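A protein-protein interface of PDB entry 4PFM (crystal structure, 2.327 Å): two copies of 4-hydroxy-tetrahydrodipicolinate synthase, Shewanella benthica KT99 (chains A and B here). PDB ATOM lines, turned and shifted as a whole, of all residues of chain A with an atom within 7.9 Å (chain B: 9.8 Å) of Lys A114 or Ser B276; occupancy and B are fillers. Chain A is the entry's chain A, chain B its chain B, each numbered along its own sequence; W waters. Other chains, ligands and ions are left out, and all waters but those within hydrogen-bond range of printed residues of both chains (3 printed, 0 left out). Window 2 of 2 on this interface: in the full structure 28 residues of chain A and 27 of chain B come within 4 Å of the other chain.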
ATOM      1  N   PRO A 111      11.335 -32.945  19.794  1.00  0.00           N
ATOM      2  CA  PRO A 111      12.435 -31.991  19.765  1.00  0.00           C
ATOM      3  C   PRO A 111      13.741 -32.598  19.194  1.00  0.00           C
ATOM      4  O   PRO A 111      13.953 -33.817  19.237  1.00  0.00           O
ATOM      5  CB  PRO A 111      12.602 -31.626  21.240  1.00  0.00           C
ATOM      6  CG  PRO A 111      12.190 -32.855  21.919  1.00  0.00           C
ATOM      7  CD  PRO A 111      11.037 -33.391  21.160  1.00  0.00           C
ATOM      8  N   SER A 112      14.592 -31.741  18.635  1.00  0.00           N
ATOM      9  CA  SER A 112      15.938 -32.203  18.216  1.00  0.00           C
ATOM     10  C   SER A 112      16.857 -32.489  19.371  1.00  0.00           C
ATOM     11  O   SER A 112      16.514 -32.171  20.528  1.00  0.00           O
ATOM     12  CB  SER A 112      16.554 -31.219  17.281  1.00  0.00           C
ATOM     13  OG  SER A 112      15.716 -31.212  16.143  1.00  0.00           O
ATOM     14  N   PRO A 113      17.981 -33.184  19.105  1.00  0.00           N
ATOM     15  CA  PRO A 113      18.878 -33.456  20.237  1.00  0.00           C
ATOM     16  C   PRO A 113      19.257 -32.193  21.021  1.00  0.00           C
ATOM     17  O   PRO A 113      19.167 -32.185  22.260  1.00  0.00           O
ATOM     18  CB  PRO A 113      20.089 -34.138  19.566  1.00  0.00           C
ATOM     19  CG  PRO A 113      19.435 -34.896  18.362  1.00  0.00           C
ATOM     20  CD  PRO A 113      18.352 -33.957  17.896  1.00  0.00           C
ATOM     21  N   LYS A 114      19.607 -31.102  20.347  1.00  0.00           N
ATOM     22  CA  LYS A 114      19.892 -29.862  21.118  1.00  0.00           C
ATOM     23  C   LYS A 114      18.728 -29.338  21.941  1.00  0.00           C
ATOM     24  O   LYS A 114      18.919 -28.719  23.018  1.00  0.00           O
ATOM     25  CB  LYS A 114      20.605 -28.737  20.323  1.00  0.00           C
ATOM     26  CG  LYS A 114      19.755 -27.903  19.397  1.00  0.00           C
ATOM     27  CD  LYS A 114      20.427 -26.495  19.027  1.00  0.00           C
ATOM     28  CE  LYS A 114      20.380 -26.211  17.492  1.00  0.00           C
ATOM     29  NZ  LYS A 114      21.654 -26.543  16.685  1.00  0.00           N
ATOM     30  N   GLY A 115      17.506 -29.604  21.474  1.00  0.00           N
ATOM     31  CA  GLY A 115      16.341 -29.219  22.253  1.00  0.00           C
ATOM     32  C   GLY A 115      16.222 -30.077  23.489  1.00  0.00           C
ATOM     33  O   GLY A 115      15.831 -29.553  24.533  1.00  0.00           O
ATOM     34  N   LEU A 116      16.564 -31.371  23.399  1.00  0.00           N
ATOM     35  CA  LEU A 116      16.496 -32.232  24.590  1.00  0.00           C
ATOM     36  C   LEU A 116      17.505 -31.732  25.610  1.00  0.00           C
ATOM     37  O   LEU A 116      17.210 -31.615  26.816  1.00  0.00           O
ATOM     38  CB  LEU A 116      16.781 -33.722  24.246  1.00  0.00           C
ATOM     39  CG  LEU A 116      15.640 -34.437  23.490  1.00  0.00           C
ATOM     40  CD1 LEU A 116      15.958 -35.828  22.884  1.00  0.00           C
ATOM     41  CD2 LEU A 116      14.412 -34.541  24.454  1.00  0.00           C
ATOM     42  N   ILE A 117      18.727 -31.472  25.129  1.00  0.00           N
ATOM     43  CA  ILE A 117      19.780 -30.934  25.994  1.00  0.00           C
ATOM     44  C   ILE A 117      19.314 -29.678  26.664  1.00  0.00           C
ATOM     45  O   ILE A 117      19.338 -29.585  27.901  1.00  0.00           O
ATOM     46  CB  ILE A 117      21.124 -30.663  25.219  1.00  0.00           C
ATOM     47  CG1 ILE A 117      21.732 -31.989  24.817  1.00  0.00           C
ATOM     48  CG2 ILE A 117      22.119 -29.919  26.143  1.00  0.00           C
ATOM     49  CD1 ILE A 117      22.719 -32.002  23.700  1.00  0.00           C
ATOM     50  N   ALA A 118      18.796 -28.733  25.887  1.00  0.00           N
ATOM     51  CA  ALA A 118      18.382 -27.449  26.484  1.00  0.00           C
ATOM     52  C   ALA A 118      17.204 -27.636  27.440  1.00  0.00           C
ATOM     53  O   ALA A 118      17.124 -26.983  28.495  1.00  0.00           O
ATOM     54  CB  ALA A 118      18.062 -26.414  25.404  1.00  0.00           C
ATOM     55  N   HIS A 119      16.270 -28.512  27.063  1.00  0.00           N
ATOM     56  CA  HIS A 119      15.128 -28.835  27.933  1.00  0.00           C
ATOM     57  C   HIS A 119      15.605 -29.332  29.281  1.00  0.00           C
ATOM     58  O   HIS A 119      15.170 -28.866  30.308  1.00  0.00           O
ATOM     59  CB  HIS A 119      14.192 -29.861  27.219  1.00  0.00           C
ATOM     60  CG  HIS A 119      13.111 -30.421  28.081  1.00  0.00           C
ATOM     61  ND1 HIS A 119      11.913 -29.765  28.303  1.00  0.00           N
ATOM     62  CD2 HIS A 119      13.047 -31.584  28.784  1.00  0.00           C
ATOM     63  CE1 HIS A 119      11.161 -30.510  29.102  1.00  0.00           C
ATOM     64  NE2 HIS A 119      11.818 -31.620  29.397  1.00  0.00           N
ATOM     65  N   TYR A 120      16.478 -30.302  29.316  1.00  0.00           N
ATOM     66  CA  TYR A 120      16.815 -30.874  30.637  1.00  0.00           C
ATOM     67  C   TYR A 120      17.764 -29.953  31.447  1.00  0.00           C
ATOM     68  O   TYR A 120      17.747 -29.968  32.689  1.00  0.00           O
ATOM     69  CB  TYR A 120      17.469 -32.215  30.446  1.00  0.00           C
ATOM     70  CG  TYR A 120      16.500 -33.372  30.206  1.00  0.00           C
ATOM     71  CD1 TYR A 120      15.573 -33.778  31.204  1.00  0.00           C
ATOM     72  CD2 TYR A 120      16.578 -34.114  29.018  1.00  0.00           C
ATOM     73  CE1 TYR A 120      14.711 -34.846  30.979  1.00  0.00           C
ATOM     74  CE2 TYR A 120      15.754 -35.181  28.792  1.00  0.00           C
ATOM     75  CZ  TYR A 120      14.805 -35.540  29.772  1.00  0.00           C
ATOM     76  OH  TYR A 120      14.045 -36.635  29.535  1.00  0.00           O
ATOM     77  N   THR A 121      18.554 -29.132  30.748  1.00  0.00           N
ATOM     78  CA  THR A 121      19.446 -28.198  31.419  1.00  0.00           C
ATOM     79  C   THR A 121      18.606 -27.175  32.151  1.00  0.00           C
ATOM     80  O   THR A 121      18.830 -26.892  33.365  1.00  0.00           O
ATOM     81  CB  THR A 121      20.421 -27.517  30.420  1.00  0.00           C
ATOM     82  OG1 THR A 121      21.270 -28.523  29.812  1.00  0.00           O
ATOM     83  CG2 THR A 121      21.256 -26.380  31.121  1.00  0.00           C
ATOM     84  N   THR A 148      23.564 -38.223  23.184  1.00  0.00           N
ATOM     85  CA  THR A 148      22.861 -37.038  23.720  1.00  0.00           C
ATOM     86  C   THR A 148      22.839 -37.052  25.246  1.00  0.00           C
ATOM     87  O   THR A 148      23.051 -36.028  25.886  1.00  0.00           O
ATOM     88  CB  THR A 148      21.437 -36.886  23.130  1.00  0.00           C
ATOM     89  OG1 THR A 148      21.528 -36.862  21.689  1.00  0.00           O
ATOM     90  CG2 THR A 148      20.786 -35.604  23.596  1.00  0.00           C
ATOM     91  N   GLN A 151      26.068 -35.625  26.842  1.00  0.00           N
ATOM     92  CA  GLN A 151      26.264 -34.175  26.945  1.00  0.00           C
ATOM     93  C   GLN A 151      25.528 -33.569  28.135  1.00  0.00           C
ATOM     94  O   GLN A 151      25.461 -32.327  28.256  1.00  0.00           O
ATOM     95  CB  GLN A 151      25.878 -33.510  25.621  1.00  0.00           C
ATOM     96  CG  GLN A 151      26.420 -34.330  24.427  1.00  0.00           C
ATOM     97  CD  GLN A 151      26.102 -33.743  23.057  1.00  0.00           C
ATOM     98  OE1 GLN A 151      26.082 -32.530  22.886  1.00  0.00           O
ATOM     99  NE2 GLN A 151      25.879 -34.615  22.066  1.00  0.00           N
ATOM    100  N   ALA B 243      11.671 -31.134   2.404  1.00  0.00           N
ATOM    101  CA  ALA B 243      12.532 -30.125   3.040  1.00  0.00           C
ATOM    102  C   ALA B 243      11.944 -29.537   4.329  1.00  0.00           C
ATOM    103  O   ALA B 243      12.664 -29.104   5.198  1.00  0.00           O
ATOM    104  CB  ALA B 243      12.857 -28.976   2.052  1.00  0.00           C
ATOM    105  N   CYS B 246      13.014 -31.544   7.720  1.00  0.00           N
ATOM    106  CA  CYS B 246      14.429 -31.921   7.970  1.00  0.00           C
ATOM    107  C   CYS B 246      14.723 -31.967   9.445  1.00  0.00           C
ATOM    108  O   CYS B 246      15.643 -32.721   9.849  1.00  0.00           O
ATOM    109  CB  CYS B 246      15.448 -31.067   7.203  1.00  0.00           C
ATOM    110  SG  CYS B 246      15.255 -29.337   7.527  1.00  0.00           S
ATOM    111  N   GLU B 247      13.997 -31.144  10.213  1.00  0.00           N
ATOM    112  CA  GLU B 247      13.773 -31.340  11.676  1.00  0.00           C
ATOM    113  C   GLU B 247      12.247 -31.357  11.866  1.00  0.00           C
ATOM    114  O   GLU B 247      11.510 -31.041  10.922  1.00  0.00           O
ATOM    115  CB  GLU B 247      14.385 -30.219  12.530  1.00  0.00           C
ATOM    116  CG  GLU B 247      15.930 -30.049  12.351  1.00  0.00           C
ATOM    117  CD  GLU B 247      16.568 -29.079  13.359  1.00  0.00           C
ATOM    118  OE1 GLU B 247      16.518 -29.310  14.580  1.00  0.00           O
ATOM    119  OE2 GLU B 247      17.134 -28.062  12.931  1.00  0.00           O
ATOM    120  N   ALA B 248      11.773 -31.765  13.041  1.00  0.00           N
ATOM    121  CA  ALA B 248      10.321 -31.907  13.305  1.00  0.00           C
ATOM    122  C   ALA B 248       9.581 -30.616  13.019  1.00  0.00           C
ATOM    123  O   ALA B 248       9.972 -29.521  13.427  1.00  0.00           O
ATOM    124  CB  ALA B 248      10.059 -32.306  14.711  1.00  0.00           C
ATOM    125  N   ILE B 251       9.509 -26.786  13.114  1.00  0.00           N
ATOM    126  CA  ILE B 251      10.867 -26.150  13.092  1.00  0.00           C
ATOM    127  C   ILE B 251      11.210 -25.514  11.734  1.00  0.00           C
ATOM    128  O   ILE B 251      11.443 -24.287  11.676  1.00  0.00           O
ATOM    129  CB  ILE B 251      11.980 -26.990  13.687  1.00  0.00           C
ATOM    130  CG1 ILE B 251      11.826 -27.005  15.213  1.00  0.00           C
ATOM    131  CG2 ILE B 251      13.452 -26.369  13.415  1.00  0.00           C
ATOM    132  CD1 ILE B 251      12.544 -28.276  15.872  1.00  0.00           C
ATOM    133  N   PRO B 252      11.157 -26.290  10.639  1.00  0.00           N
ATOM    134  CA  PRO B 252      11.535 -25.676   9.346  1.00  0.00           C
ATOM    135  C   PRO B 252      10.560 -24.654   8.779  1.00  0.00           C
ATOM    136  O   PRO B 252      10.987 -23.567   8.271  1.00  0.00           O
ATOM    137  CB  PRO B 252      11.662 -26.873   8.407  1.00  0.00           C
ATOM    138  CG  PRO B 252      11.945 -28.110   9.397  1.00  0.00           C
ATOM    139  CD  PRO B 252      11.126 -27.767  10.588  1.00  0.00           C
ATOM    140  N   TRP B 255      10.989 -21.308  10.415  1.00  0.00           N
ATOM    141  CA  TRP B 255      12.173 -20.667   9.857  1.00  0.00           C
ATOM    142  C   TRP B 255      11.876 -20.107   8.474  1.00  0.00           C
ATOM    143  O   TRP B 255      12.121 -18.928   8.225  1.00  0.00           O
ATOM    144  CB  TRP B 255      13.323 -21.671   9.789  1.00  0.00           C
ATOM    145  CG  TRP B 255      14.665 -21.043   9.502  1.00  0.00           C
ATOM    146  CD1 TRP B 255      15.581 -20.579  10.422  1.00  0.00           C
ATOM    147  CD2 TRP B 255      15.244 -20.811   8.192  1.00  0.00           C
ATOM    148  NE1 TRP B 255      16.688 -20.069   9.749  1.00  0.00           N
ATOM    149  CE2 TRP B 255      16.504 -20.203   8.393  1.00  0.00           C
ATOM    150  CE3 TRP B 255      14.812 -21.055   6.882  1.00  0.00           C
ATOM    151  CZ2 TRP B 255      17.331 -19.847   7.336  1.00  0.00           C
ATOM    152  CZ3 TRP B 255      15.647 -20.694   5.820  1.00  0.00           C
ATOM    153  CH2 TRP B 255      16.888 -20.115   6.061  1.00  0.00           C
ATOM    154  N   ILE B 268      10.572 -19.846  18.867  1.00  0.00           N
ATOM    155  CA  ILE B 268       9.871 -21.105  18.960  1.00  0.00           C
ATOM    156  C   ILE B 268      10.135 -21.558  20.376  1.00  0.00           C
ATOM    157  O   ILE B 268      11.179 -21.240  20.924  1.00  0.00           O
ATOM    158  CB  ILE B 268      10.449 -22.044  17.904  1.00  0.00           C
ATOM    159  CG1 ILE B 268       9.533 -23.216  17.600  1.00  0.00           C
ATOM    160  CG2 ILE B 268      11.844 -22.481  18.210  1.00  0.00           C
ATOM    161  CD1 ILE B 268       9.946 -23.841  16.244  1.00  0.00           C
ATOM    162  N   LEU B 270      10.744 -23.856  23.773  1.00  0.00           N
ATOM    163  CA  LEU B 270      11.408 -25.048  24.242  1.00  0.00           C
ATOM    164  C   LEU B 270      10.367 -26.126  24.569  1.00  0.00           C
ATOM    165  O   LEU B 270       9.279 -25.818  25.083  1.00  0.00           O
ATOM    166  CB  LEU B 270      12.316 -24.740  25.450  1.00  0.00           C
ATOM    167  CG  LEU B 270      13.702 -24.124  25.053  1.00  0.00           C
ATOM    168  CD1 LEU B 270      14.563 -23.583  26.247  1.00  0.00           C
ATOM    169  CD2 LEU B 270      14.554 -25.083  24.263  1.00  0.00           C
ATOM    170  N   PRO B 271      10.692 -27.389  24.279  1.00  0.00           N
ATOM    171  CA  PRO B 271      11.957 -27.959  23.800  1.00  0.00           C
ATOM    172  C   PRO B 271      12.205 -27.813  22.305  1.00  0.00           C
ATOM    173  O   PRO B 271      13.199 -28.270  21.797  1.00  0.00           O
ATOM    174  CB  PRO B 271      11.784 -29.455  24.125  1.00  0.00           C
ATOM    175  CG  PRO B 271      10.316 -29.686  24.030  1.00  0.00           C
ATOM    176  CD  PRO B 271       9.662 -28.430  24.511  1.00  0.00           C
ATOM    177  N   LEU B 272      11.285 -27.267  21.545  1.00  0.00           N
ATOM    178  CA  LEU B 272      11.594 -27.035  20.150  1.00  0.00           C
ATOM    179  C   LEU B 272      12.708 -25.933  20.069  1.00  0.00           C
ATOM    180  O   LEU B 272      12.824 -25.115  20.977  1.00  0.00           O
ATOM    181  CB  LEU B 272      10.343 -26.604  19.426  1.00  0.00           C
ATOM    182  CG  LEU B 272       9.581 -27.697  18.668  1.00  0.00           C
ATOM    183  CD1 LEU B 272       9.738 -29.083  19.277  1.00  0.00           C
ATOM    184  CD2 LEU B 272       8.114 -27.363  18.382  1.00  0.00           C
ATOM    185  N   THR B 273      13.531 -26.012  19.026  1.00  0.00           N
ATOM    186  CA  THR B 273      14.674 -25.104  18.779  1.00  0.00           C
ATOM    187  C   THR B 273      14.666 -24.614  17.352  1.00  0.00           C
ATOM    188  O   THR B 273      14.225 -25.310  16.484  1.00  0.00           O
ATOM    189  CB  THR B 273      16.054 -25.804  19.012  1.00  0.00           C
ATOM    190  OG1 THR B 273      16.088 -27.055  18.314  1.00  0.00           O
ATOM    191  CG2 THR B 273      16.289 -26.068  20.470  1.00  0.00           C
ATOM    192  N   GLU B 274      15.195 -23.434  17.103  1.00  0.00           N
ATOM    193  CA  GLU B 274      15.264 -22.886  15.747  1.00  0.00           C
ATOM    194  C   GLU B 274      16.051 -23.750  14.815  1.00  0.00           C
ATOM    195  O   GLU B 274      16.981 -24.452  15.220  1.00  0.00           O
ATOM    196  CB  GLU B 274      15.859 -21.499  15.772  1.00  0.00           C
ATOM    197  CG  GLU B 274      14.976 -20.513  16.560  1.00  0.00           C
ATOM    198  CD  GLU B 274      15.448 -19.016  16.461  1.00  0.00           C
ATOM    199  OE1 GLU B 274      16.087 -18.602  15.422  1.00  0.00           O
ATOM    200  OE2 GLU B 274      15.133 -18.262  17.429  1.00  0.00           O
ATOM    201  N   LEU B 275      15.617 -23.765  13.566  1.00  0.00           N
ATOM    202  CA  LEU B 275      16.277 -24.584  12.574  1.00  0.00           C
ATOM    203  C   LEU B 275      17.822 -24.497  12.635  1.00  0.00           C
ATOM    204  O   LEU B 275      18.425 -23.417  12.652  1.00  0.00           O
ATOM    205  CB  LEU B 275      15.763 -24.184  11.187  1.00  0.00           C
ATOM    206  CG  LEU B 275      16.209 -25.121  10.078  1.00  0.00           C
ATOM    207  CD1 LEU B 275      15.558 -26.499  10.228  1.00  0.00           C
ATOM    208  CD2 LEU B 275      15.974 -24.578   8.668  1.00  0.00           C
ATOM    209  N   SER B 276      18.439 -25.656  12.680  1.00  0.00           N
ATOM    210  CA  SER B 276      19.881 -25.808  12.662  1.00  0.00           C
ATOM    211  C   SER B 276      20.537 -25.248  11.440  1.00  0.00           C
ATOM    212  O   SER B 276      20.038 -25.457  10.332  1.00  0.00           O
ATOM    213  CB  SER B 276      20.187 -27.279  12.665  1.00  0.00           C
ATOM    214  OG  SER B 276      20.844 -27.564  13.851  1.00  0.00           O
ATOM    215  N   THR B 277      21.685 -24.595  11.635  1.00  0.00           N
ATOM    216  CA  THR B 277      22.390 -23.903  10.536  1.00  0.00           C
ATOM    217  C   THR B 277      22.661 -24.877   9.393  1.00  0.00           C
ATOM    218  O   THR B 277      22.545 -24.538   8.244  1.00  0.00           O
ATOM    219  CB  THR B 277      23.724 -23.209  10.991  1.00  0.00           C
ATOM    220  OG1 THR B 277      24.603 -24.213  11.517  1.00  0.00           O
ATOM    221  CG2 THR B 277      23.488 -22.094  12.064  1.00  0.00           C
ATOM    222  N   GLU B 278      22.958 -26.111   9.718  1.00  0.00           N
ATOM    223  CA  GLU B 278      23.210 -27.120   8.669  1.00  0.00           C
ATOM    224  C   GLU B 278      22.105 -27.363   7.647  1.00  0.00           C
ATOM    225  O   GLU B 278      22.366 -28.008   6.626  1.00  0.00           O
ATOM    226  CB  GLU B 278      23.552 -28.460   9.332  1.00  0.00           C
ATOM    227  CG  GLU B 278      23.189 -28.424  10.810  1.00  0.00           C
ATOM    228  CD  GLU B 278      22.954 -29.813  11.374  1.00  0.00           C
ATOM    229  OE1 GLU B 278      22.933 -29.925  12.650  1.00  0.00           O
ATOM    230  OE2 GLU B 278      22.809 -30.773  10.538  1.00  0.00           O
ATOM    231  N   PHE B 279      20.875 -26.893   7.908  1.00  0.00           N
ATOM    232  CA  PHE B 279      19.744 -27.173   6.989  1.00  0.00           C
ATOM    233  C   PHE B 279      19.341 -25.905   6.297  1.00  0.00           C
ATOM    234  O   PHE B 279      18.504 -25.939   5.443  1.00  0.00           O
ATOM    235  CB  PHE B 279      18.498 -27.771   7.725  1.00  0.00           C
ATOM    236  CG  PHE B 279      18.772 -29.069   8.446  1.00  0.00           C
ATOM    237  CD1 PHE B 279      19.063 -30.230   7.742  1.00  0.00           C
ATOM    238  CD2 PHE B 279      18.730 -29.134   9.838  1.00  0.00           C
ATOM    239  CE1 PHE B 279      19.310 -31.462   8.429  1.00  0.00           C
ATOM    240  CE2 PHE B 279      18.991 -30.348  10.534  1.00  0.00           C
ATOM    241  CZ  PHE B 279      19.294 -31.502   9.827  1.00  0.00           C
ATOM    242  N   HIS B 280      19.917 -24.782   6.704  1.00  0.00           N
ATOM    243  CA  HIS B 280      19.586 -23.482   6.113  1.00  0.00           C
ATOM    244  C   HIS B 280      19.651 -23.489   4.577  1.00  0.00           C
ATOM    245  O   HIS B 280      18.708 -23.098   3.890  1.00  0.00           O
ATOM    246  CB  HIS B 280      20.487 -22.408   6.698  1.00  0.00           C
ATOM    247  CG  HIS B 280      20.145 -22.018   8.109  1.00  0.00           C
ATOM    248  ND1 HIS B 280      20.566 -20.836   8.672  1.00  0.00           N
ATOM    249  CD2 HIS B 280      19.398 -22.636   9.062  1.00  0.00           C
ATOM    250  CE1 HIS B 280      20.115 -20.745   9.912  1.00  0.00           C
ATOM    251  NE2 HIS B 280      19.399 -21.822  10.172  1.00  0.00           N
ATOM    252  N   GLY B 281      20.756 -23.991   4.029  1.00  0.00           N
ATOM    253  CA  GLY B 281      21.004 -23.917   2.586  1.00  0.00           C
ATOM    254  C   GLY B 281      20.055 -24.852   1.892  1.00  0.00           C
ATOM    255  O   GLY B 281      19.466 -24.514   0.853  1.00  0.00           O
ATOM    256  N   LEU B 282      19.877 -26.018   2.476  1.00  0.00           N
ATOM    257  CA  LEU B 282      18.922 -26.955   1.927  1.00  0.00           C
ATOM    258  C   LEU B 282      17.512 -26.356   1.807  1.00  0.00           C
ATOM    259  O   LEU B 282      16.879 -26.392   0.724  1.00  0.00           O
ATOM    260  CB  LEU B 282      18.938 -28.231   2.762  1.00  0.00           C
ATOM    261  CG  LEU B 282      17.857 -29.314   2.714  1.00  0.00           C
ATOM    262  CD1 LEU B 282      17.445 -29.714   1.296  1.00  0.00           C
ATOM    263  CD2 LEU B 282      18.433 -30.516   3.465  1.00  0.00           C
ATOM    264  N   LEU B 283      16.996 -25.794   2.889  1.00  0.00           N
ATOM    265  CA  LEU B 283      15.623 -25.250   2.800  1.00  0.00           C
ATOM    266  C   LEU B 283      15.528 -23.952   1.961  1.00  0.00           C
ATOM    267  O   LEU B 283      14.579 -23.755   1.232  1.00  0.00           O
ATOM    268  CB  LEU B 283      15.013 -25.093   4.206  1.00  0.00           C
ATOM    269  CG  LEU B 283      13.666 -24.446   4.492  1.00  0.00           C
ATOM    270  CD1 LEU B 283      12.525 -25.199   3.830  1.00  0.00           C
ATOM    271  CD2 LEU B 283      13.535 -24.469   5.985  1.00  0.00           C
ATOM    272  N   LEU B 284      16.513 -23.075   2.067  1.00  0.00           N
ATOM    273  CA  LEU B 284      16.522 -21.883   1.222  1.00  0.00           C
ATOM    274  C   LEU B 284      16.436 -22.291  -0.269  1.00  0.00           C
ATOM    275  O   LEU B 284      15.669 -21.701  -1.026  1.00  0.00           O
ATOM    276  CB  LEU B 284      17.741 -21.008   1.515  1.00  0.00           C
ATOM    277  CG  LEU B 284      17.356 -19.522   1.562  1.00  0.00           C
ATOM    278  CD1 LEU B 284      17.329 -19.091   2.992  1.00  0.00           C
ATOM    279  CD2 LEU B 284      18.305 -18.520   0.758  1.00  0.00           C
HETATM  280  O   HOH W   1      14.178 -28.931  19.367  1.00  0.00           O
HETATM  281  O   HOH W   2      13.198 -32.296  15.559  1.00  0.00           O
HETATM  282  O   HOH W   3      22.320 -24.197  14.560  1.00  0.00           O
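OG of Ser A112 lies within hydrogen-bond range of OE1 of Glu B247, at 2.6 Å.
The side-chain amino group (NZ) of Lys A114 lies within hydrogen-bond range of the side-chain hydroxyl (OG) of Ser B276 (3.1 Å).
The side-chain carboxylate of Glu B247 lies within hydrogen-bond range of the backbone NH of Ser B276, at 2.7 Å.
OE1 of Glu B278 lies within hydrogen-bond range of OG of Ser B276, 3.4 Å away.
Pro A111 touches Pro B271.
CA of Pro A111 touches CD1 of Leu B272, at 3.996 Å.
Thr B273 touches Lys A114 (OG1 to CG, 3.9 Å).
Pro B271 touches Gly A115 (O to CA, 3.3 Å).
Gly A115 touches Thr B273.
Ala A118 touches Leu B270 (CB to CD2, 3.9 Å).
CB of His A119 touches CB of Pro B271, at 3.9 Å.
Of chain A, only Lys A114 (3.1 Å) comes within 4 Å of Ser B276.
Of the printed residues of chain B, Ser A112 touches Glu B247.
Pro A113 touches none of the printed residues of chain B.
Of the printed residues of chain B, Gly A115 touches Pro B271 and Thr B273.
Printed residues of chain B within 4 Å of Pro A111: Pro B271 and Leu B272.
Printed residues of chain A within 4 Å of Glu B247: Ser A112.
The nearest residue of chain B that does not touch Lys A114 is Glu B274 (4.5 Å).
The nearest printed residue of chain A that does not touch Leu B272 is Gly A115 (5.4 Å).
Of the 23 printed residues of chain B, 6 touch a printed residue of chain A.
Printed residues of chain B that touch a printed residue of chain A: Glu B247, Leu B270, Pro B271, Leu B272, Thr B273 and Ser B276.
Hydrophobic or aromatic side chains of chain B that line the printed part of chain A: Leu B270, Pro B271 and Leu B272.
Among the printed residues, no Asp or Glu carboxylate lies within 4 Å of a Lys or Arg side-chain nitrogen of the other chain.
No position is printed for both chains.
Of the 9 pairs that touch across the chains among the printed residues, none has its exchanged pair printed and touching as well.
Water W1 lies within hydrogen-bond range of O of Pro B271 (2.7 Å), OG1 of Thr B273 (2.9 Å) and N of Ser A112 (2.9 Å).
Water W2 lies within hydrogen-bond range of the side-chain hydroxyl (OG) of Ser A112 (2.8 Å) and the backbone NH (N) of Ala B248 (2.9 Å).
Water W3 bridges N of Thr B277 and NZ of Lys A114.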
